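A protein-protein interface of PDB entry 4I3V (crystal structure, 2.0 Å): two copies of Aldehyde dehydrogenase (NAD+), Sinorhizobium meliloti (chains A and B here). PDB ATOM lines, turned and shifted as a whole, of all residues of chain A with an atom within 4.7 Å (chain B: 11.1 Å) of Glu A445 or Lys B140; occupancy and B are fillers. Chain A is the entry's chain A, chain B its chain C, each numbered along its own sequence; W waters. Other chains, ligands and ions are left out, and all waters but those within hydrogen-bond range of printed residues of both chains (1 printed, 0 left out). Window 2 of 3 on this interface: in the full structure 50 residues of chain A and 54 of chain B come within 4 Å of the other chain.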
ATOM      1  N   LEU A 264      -2.576  -8.841  19.259  1.00  0.00           N
ATOM      2  CA  LEU A 264      -2.336  -8.184  17.992  1.00  0.00           C
ATOM      3  C   LEU A 264      -1.573  -6.920  18.345  1.00  0.00           C
ATOM      4  O   LEU A 264      -2.062  -6.070  19.094  1.00  0.00           O
ATOM      5  CB  LEU A 264      -3.648  -7.835  17.293  1.00  0.00           C
ATOM      6  CG  LEU A 264      -3.442  -7.151  15.940  1.00  0.00           C
ATOM      7  CD1 LEU A 264      -2.749  -8.107  15.007  1.00  0.00           C
ATOM      8  CD2 LEU A 264      -4.770  -6.657  15.324  1.00  0.00           C
ATOM      9  N   LEU A 281      -8.109  -5.705  11.154  1.00  0.00           N
ATOM     10  CA  LEU A 281      -7.543  -6.906  11.756  1.00  0.00           C
ATOM     11  C   LEU A 281      -7.946  -7.055  13.213  1.00  0.00           C
ATOM     12  O   LEU A 281      -8.370  -8.137  13.637  1.00  0.00           O
ATOM     13  CB  LEU A 281      -6.018  -6.909  11.626  1.00  0.00           C
ATOM     14  CG  LEU A 281      -5.498  -7.142  10.205  1.00  0.00           C
ATOM     15  CD1 LEU A 281      -3.960  -7.180  10.181  1.00  0.00           C
ATOM     16  CD2 LEU A 281      -6.069  -8.436   9.641  1.00  0.00           C
ATOM     17  N   GLY A 420      -0.029 -11.626  16.291  1.00  0.00           N
ATOM     18  CA  GLY A 420      -0.009 -10.878  15.050  1.00  0.00           C
ATOM     19  C   GLY A 420       0.698  -9.558  15.303  1.00  0.00           C
ATOM     20  O   GLY A 420       0.591  -8.984  16.394  1.00  0.00           O
ATOM     21  N   VAL A 421       1.437  -9.080  14.312  1.00  0.00           N
ATOM     22  CA  VAL A 421       2.172  -7.829  14.458  1.00  0.00           C
ATOM     23  C   VAL A 421       2.025  -6.968  13.212  1.00  0.00           C
ATOM     24  O   VAL A 421       2.328  -7.415  12.108  1.00  0.00           O
ATOM     25  CB  VAL A 421       3.680  -8.098  14.694  1.00  0.00           C
ATOM     26  CG1 VAL A 421       4.428  -6.799  14.941  1.00  0.00           C
ATOM     27  CG2 VAL A 421       3.861  -9.039  15.866  1.00  0.00           C
ATOM     28  N   ASN A 442       2.444 -13.953  13.221  1.00  0.00           N
ATOM     29  CA  ASN A 442       1.945 -13.537  11.912  1.00  0.00           C
ATOM     30  C   ASN A 442       2.161 -12.050  11.661  1.00  0.00           C
ATOM     31  O   ASN A 442       1.670 -11.219  12.416  1.00  0.00           O
ATOM     32  CB  ASN A 442       0.459 -13.860  11.748  1.00  0.00           C
ATOM     33  CG  ASN A 442       0.201 -15.344  11.609  1.00  0.00           C
ATOM     34  OD1 ASN A 442       0.957 -16.060  10.945  1.00  0.00           O
ATOM     35  ND2 ASN A 442      -0.861 -15.816  12.241  1.00  0.00           N
ATOM     36  N   ILE A 443       2.885 -11.716  10.600  1.00  0.00           N
ATOM     37  CA  ILE A 443       3.045 -10.305  10.238  1.00  0.00           C
ATOM     38  C   ILE A 443       1.870  -9.837   9.386  1.00  0.00           C
ATOM     39  O   ILE A 443       1.624 -10.379   8.308  1.00  0.00           O
ATOM     40  CB  ILE A 443       4.362 -10.045   9.483  1.00  0.00           C
ATOM     41  CG1 ILE A 443       5.558 -10.428  10.365  1.00  0.00           C
ATOM     42  CG2 ILE A 443       4.434  -8.573   9.038  1.00  0.00           C
ATOM     43  CD1 ILE A 443       5.506  -9.855  11.744  1.00  0.00           C
ATOM     44  N   TRP A 444       1.159  -8.819   9.872  1.00  0.00           N
ATOM     45  CA  TRP A 444       0.022  -8.258   9.146  1.00  0.00           C
ATOM     46  C   TRP A 444      -1.130  -9.254   8.979  1.00  0.00           C
ATOM     47  O   TRP A 444      -1.789  -9.306   7.942  1.00  0.00           O
ATOM     48  CB  TRP A 444       0.472  -7.685   7.795  1.00  0.00           C
ATOM     49  CG  TRP A 444       0.798  -6.208   7.895  1.00  0.00           C
ATOM     50  CD1 TRP A 444       2.008  -5.610   7.671  1.00  0.00           C
ATOM     51  CD2 TRP A 444      -0.097  -5.164   8.295  1.00  0.00           C
ATOM     52  NE1 TRP A 444       1.913  -4.249   7.888  1.00  0.00           N
ATOM     53  CE2 TRP A 444       0.628  -3.952   8.274  1.00  0.00           C
ATOM     54  CE3 TRP A 444      -1.451  -5.133   8.661  1.00  0.00           C
ATOM     55  CZ2 TRP A 444       0.049  -2.723   8.601  1.00  0.00           C
ATOM     56  CZ3 TRP A 444      -2.023  -3.913   8.994  1.00  0.00           C
ATOM     57  CH2 TRP A 444      -1.273  -2.724   8.958  1.00  0.00           C
ATOM     58  N   GLU A 445      -1.358 -10.054  10.006  1.00  0.00           N
ATOM     59  CA  GLU A 445      -2.523 -10.930  10.040  1.00  0.00           C
ATOM     60  C   GLU A 445      -2.851 -11.156  11.489  1.00  0.00           C
ATOM     61  O   GLU A 445      -2.026 -10.899  12.357  1.00  0.00           O
ATOM     62  CB  GLU A 445      -2.253 -12.277   9.358  1.00  0.00           C
ATOM     63  CG  GLU A 445      -2.896 -12.440   7.968  1.00  0.00           C
ATOM     64  CD  GLU A 445      -4.435 -12.350   7.980  1.00  0.00           C
ATOM     65  OE1 GLU A 445      -5.051 -12.415   9.064  1.00  0.00           O
ATOM     66  OE2 GLU A 445      -5.027 -12.214   6.892  1.00  0.00           O
ATOM     67  N   VAL A 446      -4.053 -11.645  11.743  1.00  0.00           N
ATOM     68  CA  VAL A 446      -4.478 -11.992  13.082  1.00  0.00           C
ATOM     69  C   VAL A 446      -3.733 -13.237  13.540  1.00  0.00           C
ATOM     70  O   VAL A 446      -3.288 -14.037  12.716  1.00  0.00           O
ATOM     71  CB  VAL A 446      -5.984 -12.287  13.088  1.00  0.00           C
ATOM     72  CG1 VAL A 446      -6.762 -11.046  12.683  1.00  0.00           C
ATOM     73  CG2 VAL A 446      -6.298 -13.429  12.133  1.00  0.00           C
ATOM     74  N   PRO A 447      -3.610 -13.426  14.865  1.00  0.00           N
ATOM     75  CA  PRO A 447      -2.911 -14.611  15.386  1.00  0.00           C
ATOM     76  C   PRO A 447      -3.498 -15.919  14.852  1.00  0.00           C
ATOM     77  O   PRO A 447      -2.763 -16.874  14.629  1.00  0.00           O
ATOM     78  CB  PRO A 447      -3.139 -14.525  16.897  1.00  0.00           C
ATOM     79  CG  PRO A 447      -3.406 -13.086  17.170  1.00  0.00           C
ATOM     80  CD  PRO A 447      -4.117 -12.555  15.938  1.00  0.00           C
ATOM     81  N   TYR A 449      -4.531 -16.739  12.033  1.00  0.00           N
ATOM     82  CA  TYR A 449      -4.290 -17.088  10.650  1.00  0.00           C
ATOM     83  C   TYR A 449      -3.329 -18.274  10.492  1.00  0.00           C
ATOM     84  O   TYR A 449      -2.222 -18.256  11.021  1.00  0.00           O
ATOM     85  CB  TYR A 449      -3.759 -15.919   9.798  1.00  0.00           C
ATOM     86  CG  TYR A 449      -3.514 -16.492   8.432  1.00  0.00           C
ATOM     87  CD1 TYR A 449      -4.576 -16.703   7.561  1.00  0.00           C
ATOM     88  CD2 TYR A 449      -2.263 -16.964   8.064  1.00  0.00           C
ATOM     89  CE1 TYR A 449      -4.386 -17.294   6.324  1.00  0.00           C
ATOM     90  CE2 TYR A 449      -2.060 -17.561   6.823  1.00  0.00           C
ATOM     91  CZ  TYR A 449      -3.128 -17.724   5.954  1.00  0.00           C
ATOM     92  OH  TYR A 449      -2.956 -18.327   4.712  1.00  0.00           O
ATOM     93  N   PHE B 131       5.875 -22.700   3.430  1.00  0.00           N
ATOM     94  CA  PHE B 131       4.566 -23.004   2.859  1.00  0.00           C
ATOM     95  C   PHE B 131       4.005 -21.802   2.088  1.00  0.00           C
ATOM     96  O   PHE B 131       4.049 -20.654   2.568  1.00  0.00           O
ATOM     97  CB  PHE B 131       3.552 -23.399   3.949  1.00  0.00           C
ATOM     98  CG  PHE B 131       3.920 -24.635   4.722  1.00  0.00           C
ATOM     99  CD1 PHE B 131       3.325 -25.861   4.433  1.00  0.00           C
ATOM    100  CD2 PHE B 131       4.845 -24.572   5.761  1.00  0.00           C
ATOM    101  CE1 PHE B 131       3.666 -27.011   5.158  1.00  0.00           C
ATOM    102  CE2 PHE B 131       5.197 -25.722   6.490  1.00  0.00           C
ATOM    103  CZ  PHE B 131       4.604 -26.933   6.195  1.00  0.00           C
ATOM    104  N   SER B 132       3.468 -22.069   0.902  1.00  0.00           N
ATOM    105  CA  SER B 132       2.704 -21.069   0.171  1.00  0.00           C
ATOM    106  C   SER B 132       1.270 -21.136   0.669  1.00  0.00           C
ATOM    107  O   SER B 132       0.750 -22.218   0.897  1.00  0.00           O
ATOM    108  CB  SER B 132       2.743 -21.324  -1.335  1.00  0.00           C
ATOM    109  OG  SER B 132       4.010 -21.006  -1.880  1.00  0.00           O
ATOM    110  N   CYS B 133       0.626 -19.984   0.820  1.00  0.00           N
ATOM    111  CA  CYS B 133      -0.677 -19.939   1.469  1.00  0.00           C
ATOM    112  C   CYS B 133      -1.867 -19.844   0.513  1.00  0.00           C
ATOM    113  O   CYS B 133      -3.002 -19.836   0.961  1.00  0.00           O
ATOM    114  CB  CYS B 133      -0.724 -18.767   2.448  1.00  0.00           C
ATOM    115  SG  CYS B 133       0.285 -19.032   3.932  1.00  0.00           S
ATOM    116  N   ASP B 134      -1.616 -19.768  -0.789  1.00  0.00           N
ATOM    117  CA  ASP B 134      -2.703 -19.522  -1.751  1.00  0.00           C
ATOM    118  C   ASP B 134      -3.249 -20.827  -2.351  1.00  0.00           C
ATOM    119  O   ASP B 134      -3.231 -21.011  -3.565  1.00  0.00           O
ATOM    120  CB  ASP B 134      -2.254 -18.539  -2.853  1.00  0.00           C
ATOM    121  CG  ASP B 134      -1.016 -19.021  -3.613  1.00  0.00           C
ATOM    122  OD1 ASP B 134      -0.107 -19.573  -2.974  1.00  0.00           O
ATOM    123  OD2 ASP B 134      -0.943 -18.859  -4.848  1.00  0.00           O
ATOM    124  N   LEU B 135      -3.761 -21.709  -1.491  1.00  0.00           N
ATOM    125  CA  LEU B 135      -3.973 -23.119  -1.847  1.00  0.00           C
ATOM    126  C   LEU B 135      -5.428 -23.570  -1.925  1.00  0.00           C
ATOM    127  O   LEU B 135      -5.724 -24.638  -2.463  1.00  0.00           O
ATOM    128  CB  LEU B 135      -3.301 -24.019  -0.807  1.00  0.00           C
ATOM    129  CG  LEU B 135      -1.881 -23.698  -0.359  1.00  0.00           C
ATOM    130  CD1 LEU B 135      -1.403 -24.816   0.558  1.00  0.00           C
ATOM    131  CD2 LEU B 135      -0.970 -23.561  -1.580  1.00  0.00           C
ATOM    132  N   THR B 136      -6.315 -22.793  -1.323  1.00  0.00           N
ATOM    133  CA  THR B 136      -7.705 -23.182  -1.159  1.00  0.00           C
ATOM    134  C   THR B 136      -8.530 -21.907  -1.297  1.00  0.00           C
ATOM    135  O   THR B 136      -7.956 -20.834  -1.472  1.00  0.00           O
ATOM    136  CB  THR B 136      -7.949 -23.840   0.224  1.00  0.00           C
ATOM    137  OG1 THR B 136      -7.922 -22.848   1.256  1.00  0.00           O
ATOM    138  CG2 THR B 136      -6.894 -24.897   0.521  1.00  0.00           C
ATOM    139  N   PRO B 137      -9.869 -22.018  -1.229  1.00  0.00           N
ATOM    140  CA  PRO B 137     -10.694 -20.807  -1.278  1.00  0.00           C
ATOM    141  C   PRO B 137     -10.388 -19.860  -0.121  1.00  0.00           C
ATOM    142  O   PRO B 137     -10.705 -18.679  -0.218  1.00  0.00           O
ATOM    143  CB  PRO B 137     -12.130 -21.352  -1.158  1.00  0.00           C
ATOM    144  CG  PRO B 137     -12.044 -22.737  -1.679  1.00  0.00           C
ATOM    145  CD  PRO B 137     -10.690 -23.242  -1.245  1.00  0.00           C
ATOM    146  N   HIS B 138      -9.793 -20.369   0.957  1.00  0.00           N
ATOM    147  CA  HIS B 138      -9.441 -19.530   2.105  1.00  0.00           C
ATOM    148  C   HIS B 138      -8.022 -18.968   1.967  1.00  0.00           C
ATOM    149  O   HIS B 138      -7.520 -18.317   2.885  1.00  0.00           O
ATOM    150  CB  HIS B 138      -9.560 -20.309   3.425  1.00  0.00           C
ATOM    151  CG  HIS B 138     -10.967 -20.515   3.894  1.00  0.00           C
ATOM    152  ND1 HIS B 138     -11.273 -21.177   5.065  1.00  0.00           N
ATOM    153  CD2 HIS B 138     -12.155 -20.144   3.353  1.00  0.00           C
ATOM    154  CE1 HIS B 138     -12.580 -21.196   5.231  1.00  0.00           C
ATOM    155  NE2 HIS B 138     -13.142 -20.579   4.209  1.00  0.00           N
ATOM    156  N   GLY B 139      -7.384 -19.221   0.824  1.00  0.00           N
ATOM    157  CA  GLY B 139      -5.988 -18.848   0.610  1.00  0.00           C
ATOM    158  C   GLY B 139      -5.660 -17.357   0.665  1.00  0.00           C
ATOM    159  O   GLY B 139      -6.525 -16.522   0.454  1.00  0.00           O
ATOM    160  N   LYS B 140      -4.401 -17.033   0.956  1.00  0.00           N
ATOM    161  CA  LYS B 140      -3.918 -15.646   0.982  1.00  0.00           C
ATOM    162  C   LYS B 140      -2.595 -15.554   0.220  1.00  0.00           C
ATOM    163  O   LYS B 140      -1.918 -16.560   0.036  1.00  0.00           O
ATOM    164  CB  LYS B 140      -3.688 -15.172   2.417  1.00  0.00           C
ATOM    165  CG  LYS B 140      -4.909 -15.207   3.313  1.00  0.00           C
ATOM    166  CD  LYS B 140      -5.870 -14.106   2.981  1.00  0.00           C
ATOM    167  CE  LYS B 140      -7.073 -14.120   3.922  1.00  0.00           C
ATOM    168  NZ  LYS B 140      -6.707 -13.832   5.340  1.00  0.00           N
ATOM    169  N   ALA B 141      -2.226 -14.349  -0.214  1.00  0.00           N
ATOM    170  CA  ALA B 141      -0.941 -14.129  -0.869  1.00  0.00           C
ATOM    171  C   ALA B 141       0.112 -13.940   0.220  1.00  0.00           C
ATOM    172  O   ALA B 141       0.376 -12.822   0.672  1.00  0.00           O
ATOM    173  CB  ALA B 141      -1.007 -12.903  -1.776  1.00  0.00           C
ATOM    174  N   ARG B 142       0.707 -15.044   0.644  1.00  0.00           N
ATOM    175  CA  ARG B 142       1.435 -15.080   1.903  1.00  0.00           C
ATOM    176  C   ARG B 142       2.307 -16.328   1.947  1.00  0.00           C
ATOM    177  O   ARG B 142       2.016 -17.314   1.285  1.00  0.00           O
ATOM    178  CB  ARG B 142       0.418 -15.054   3.064  1.00  0.00           C
ATOM    179  CG  ARG B 142       0.962 -15.320   4.464  1.00  0.00           C
ATOM    180  CD  ARG B 142      -0.065 -14.955   5.527  1.00  0.00           C
ATOM    181  NE  ARG B 142      -0.391 -13.522   5.509  1.00  0.00           N
ATOM    182  CZ  ARG B 142       0.206 -12.600   6.267  1.00  0.00           C
ATOM    183  NH1 ARG B 142       1.164 -12.953   7.123  1.00  0.00           N
ATOM    184  NH2 ARG B 142      -0.158 -11.319   6.186  1.00  0.00           N
ATOM    185  N   LYS B 143       3.397 -16.271   2.696  1.00  0.00           N
ATOM    186  CA  LYS B 143       4.241 -17.447   2.886  1.00  0.00           C
ATOM    187  C   LYS B 143       4.394 -17.672   4.376  1.00  0.00           C
ATOM    188  O   LYS B 143       4.476 -16.707   5.148  1.00  0.00           O
ATOM    189  CB  LYS B 143       5.635 -17.253   2.278  1.00  0.00           C
ATOM    190  CG  LYS B 143       5.707 -17.282   0.783  1.00  0.00           C
ATOM    191  CD  LYS B 143       7.156 -17.072   0.356  1.00  0.00           C
ATOM    192  CE  LYS B 143       7.297 -17.009  -1.164  1.00  0.00           C
ATOM    193  NZ  LYS B 143       6.754 -18.236  -1.800  1.00  0.00           N
ATOM    194  N   ILE B 144       4.428 -18.946   4.762  1.00  0.00           N
ATOM    195  CA  ILE B 144       4.744 -19.343   6.125  1.00  0.00           C
ATOM    196  C   ILE B 144       6.141 -19.961   6.161  1.00  0.00           C
ATOM    197  O   ILE B 144       6.518 -20.764   5.288  1.00  0.00           O
ATOM    198  CB  ILE B 144       3.708 -20.351   6.679  1.00  0.00           C
ATOM    199  CG1 ILE B 144       2.311 -19.718   6.709  1.00  0.00           C
ATOM    200  CG2 ILE B 144       4.132 -20.864   8.054  1.00  0.00           C
ATOM    201  CD1 ILE B 144       1.166 -20.724   6.949  1.00  0.00           C
ATOM    202  N   THR B 482       6.724 -20.901  13.882  1.00  0.00           N
ATOM    203  CA  THR B 482       6.446 -20.481  12.517  1.00  0.00           C
ATOM    204  C   THR B 482       6.259 -18.961  12.458  1.00  0.00           C
ATOM    205  O   THR B 482       5.902 -18.314  13.455  1.00  0.00           O
ATOM    206  CB  THR B 482       5.195 -21.179  11.936  1.00  0.00           C
ATOM    207  OG1 THR B 482       4.016 -20.531  12.426  1.00  0.00           O
ATOM    208  CG2 THR B 482       5.179 -22.660  12.325  1.00  0.00           C
ATOM    209  N   PHE B 483       6.526 -18.384  11.299  1.00  0.00           N
ATOM    210  CA  PHE B 483       6.117 -17.002  11.065  1.00  0.00           C
ATOM    211  C   PHE B 483       5.649 -16.856   9.626  1.00  0.00           C
ATOM    212  O   PHE B 483       6.051 -17.636   8.755  1.00  0.00           O
ATOM    213  CB  PHE B 483       7.224 -15.999  11.416  1.00  0.00           C
ATOM    214  CG  PHE B 483       8.476 -16.160  10.617  1.00  0.00           C
ATOM    215  CD1 PHE B 483       9.442 -17.080  10.995  1.00  0.00           C
ATOM    216  CD2 PHE B 483       8.701 -15.375   9.490  1.00  0.00           C
ATOM    217  CE1 PHE B 483      10.618 -17.221  10.265  1.00  0.00           C
ATOM    218  CE2 PHE B 483       9.866 -15.511   8.743  1.00  0.00           C
ATOM    219  CZ  PHE B 483      10.835 -16.435   9.139  1.00  0.00           C
ATOM    220  N   SER B 484       4.768 -15.889   9.395  1.00  0.00           N
ATOM    221  CA  SER B 484       4.200 -15.659   8.069  1.00  0.00           C
ATOM    222  C   SER B 484       4.331 -14.194   7.674  1.00  0.00           C
ATOM    223  O   SER B 484       4.190 -13.307   8.513  1.00  0.00           O
ATOM    224  CB  SER B 484       2.728 -16.111   7.999  1.00  0.00           C
ATOM    225  OG  SER B 484       1.856 -15.243   8.719  1.00  0.00           O
ATOM    226  N   LEU B 485       4.613 -13.967   6.392  1.00  0.00           N
ATOM    227  CA  LEU B 485       4.865 -12.642   5.841  1.00  0.00           C
ATOM    228  C   LEU B 485       3.962 -12.421   4.628  1.00  0.00           C
ATOM    229  O   LEU B 485       3.714 -13.351   3.861  1.00  0.00           O
ATOM    230  CB  LEU B 485       6.334 -12.531   5.383  1.00  0.00           C
ATOM    231  CG  LEU B 485       7.452 -12.785   6.410  1.00  0.00           C
ATOM    232  CD1 LEU B 485       8.834 -12.699   5.740  1.00  0.00           C
ATOM    233  CD2 LEU B 485       7.359 -11.790   7.577  1.00  0.00           C
ATOM    234  N   PRO B 486       3.479 -11.180   4.446  1.00  0.00           N
ATOM    235  CA  PRO B 486       2.793 -10.792   3.211  1.00  0.00           C
ATOM    236  C   PRO B 486       3.640 -11.116   1.980  1.00  0.00           C
ATOM    237  O   PRO B 486       4.848 -10.861   1.981  1.00  0.00           O
ATOM    238  CB  PRO B 486       2.644  -9.272   3.365  1.00  0.00           C
ATOM    239  CG  PRO B 486       2.596  -9.058   4.853  1.00  0.00           C
ATOM    240  CD  PRO B 486       3.555 -10.064   5.411  1.00  0.00           C
ATOM    241  N   TRP B 487       3.024 -11.692   0.952  1.00  0.00           N
ATOM    242  CA  TRP B 487       3.763 -12.044  -0.262  1.00  0.00           C
ATOM    243  C   TRP B 487       2.962 -11.827  -1.555  1.00  0.00           C
ATOM    244  O   TRP B 487       2.570 -12.793  -2.203  1.00  0.00           O
ATOM    245  CB  TRP B 487       4.286 -13.480  -0.197  1.00  0.00           C
ATOM    246  CG  TRP B 487       5.556 -13.628  -0.985  1.00  0.00           C
ATOM    247  CD1 TRP B 487       5.668 -13.944  -2.306  1.00  0.00           C
ATOM    248  CD2 TRP B 487       6.887 -13.410  -0.514  1.00  0.00           C
ATOM    249  NE1 TRP B 487       6.985 -13.957  -2.682  1.00  0.00           N
ATOM    250  CE2 TRP B 487       7.764 -13.627  -1.590  1.00  0.00           C
ATOM    251  CE3 TRP B 487       7.436 -13.056   0.725  1.00  0.00           C
ATOM    252  CZ2 TRP B 487       9.144 -13.506  -1.485  1.00  0.00           C
ATOM    253  CZ3 TRP B 487       8.815 -12.941   0.839  1.00  0.00           C
ATOM    254  CH2 TRP B 487       9.652 -13.172  -0.256  1.00  0.00           C
HETATM  255  O   HOH W   1      -5.435 -19.803   3.925  1.00  0.00           O
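No residue of chain B comes within 4 Å of Gly A420. Printed residues of chain B within 4 Å of Asn A442: Ser B484. Of the printed residues of chain B, Ile A443 touches Arg B142, Ser B484, Leu B485 and Pro B486. Of the printed residues of chain B, Trp A444 touches Arg B142 (3.1 Å) and Pro B486 (3.9 Å). Glu A445 touches just these residues of chain B: Lys B140 and Arg B142. No residue of chain B comes within 4 Å of Val A446. No residue of chain B comes within 4 Å of Pro A447. Thr B136 touches none of the printed residues of chain A. Lys B140 touches two residues of chain A. Of the printed residues of chain A, Arg B142 touches Ile A443 (2.9 Å), Trp A444 (3.1 Å), Glu A445 (3.5 Å) and Tyr A449 (3.5 Å). Of the printed residues of chain A, Leu B485 touches Ile A443. Printed residues of chain A within 4 Å of Pro B486: Ile A443 (3.5 Å) and Trp A444 (3.9 Å). The nearest residue of chain B that does not touch Glu A445 is Ser B484 (5.1 Å). The nearest printed residue of chain B that does not touch Ile A443 is Phe B483 (5.9 Å).
Of the 20 printed residues of chain B, 6 touch a printed residue of chain A. Hydrophobic or aromatic side chains of chain B that line the printed part of chain A: Leu B485 and Pro B486. Of the 11 printed residues of chain A, 5 touch a printed residue of chain B.
N of Cys B133 sits at hydrogen-bond distance from O of Arg B142, 3.0 Å away. N of Asp B134 is in hydrogen-bond range of O of Lys B140. The backbone carbonyl oxygen (O) of Pro A447 is in hydrogen-bond range of the side-chain amide nitrogen (ND2) of Asn A442, 3.2 Å away. The backbone carbonyl oxygen of Cys B133 sits at hydrogen-bond distance from the backbone NH of Lys B140. The side-chain amide nitrogen of Asn A442 lies within hydrogen-bond range of the backbone carbonyl oxygen of Val A446, at 3.0 Å. The backbone carbonyl oxygen (O) of Tyr A449 is in hydrogen-bond range of the side-chain amide nitrogen (ND2) of Asn A442, 3.0 Å away.
Water W1 lies within hydrogen-bond range of O of His B138 (2.8 Å) and OH of Tyr A449 (3.0 Å).
O of Ser B484 lies within hydrogen-bond range of N of Ile A443 (2.9 Å). OH of Tyr A449 sits close to SG of Cys B133 (3.4 Å). The guanidinium group (NH1) of Arg B142 sits at hydrogen-bond distance from the backbone carbonyl oxygen (O) of Ile A443 (2.9 Å). OE2 of Glu A445 lies within salt-bridge range of NZ of Lys B140, 2.8 Å away. O of Trp A444 is in hydrogen-bond range of NH2 of Arg B142 (3.1 Å). The side-chain amide oxygen (OD1) of Asn A442 sits at hydrogen-bond distance from the side-chain hydroxyl (OG) of Ser B484, at 2.5 Å.
No position is printed for both chains.
Ile A443 touches Leu B485. Ile A443 touches Pro B486 (O to CD, 3.5 Å). Pro B486 touches Trp A444 (CG to CB, 3.9 Å). NH2 of Arg B142 touches CG of Glu A445 (3.5 Å). Lys B140 touches Tyr A449. Tyr A449 touches Arg B142 (CE2 to CD, 3.5 Å).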
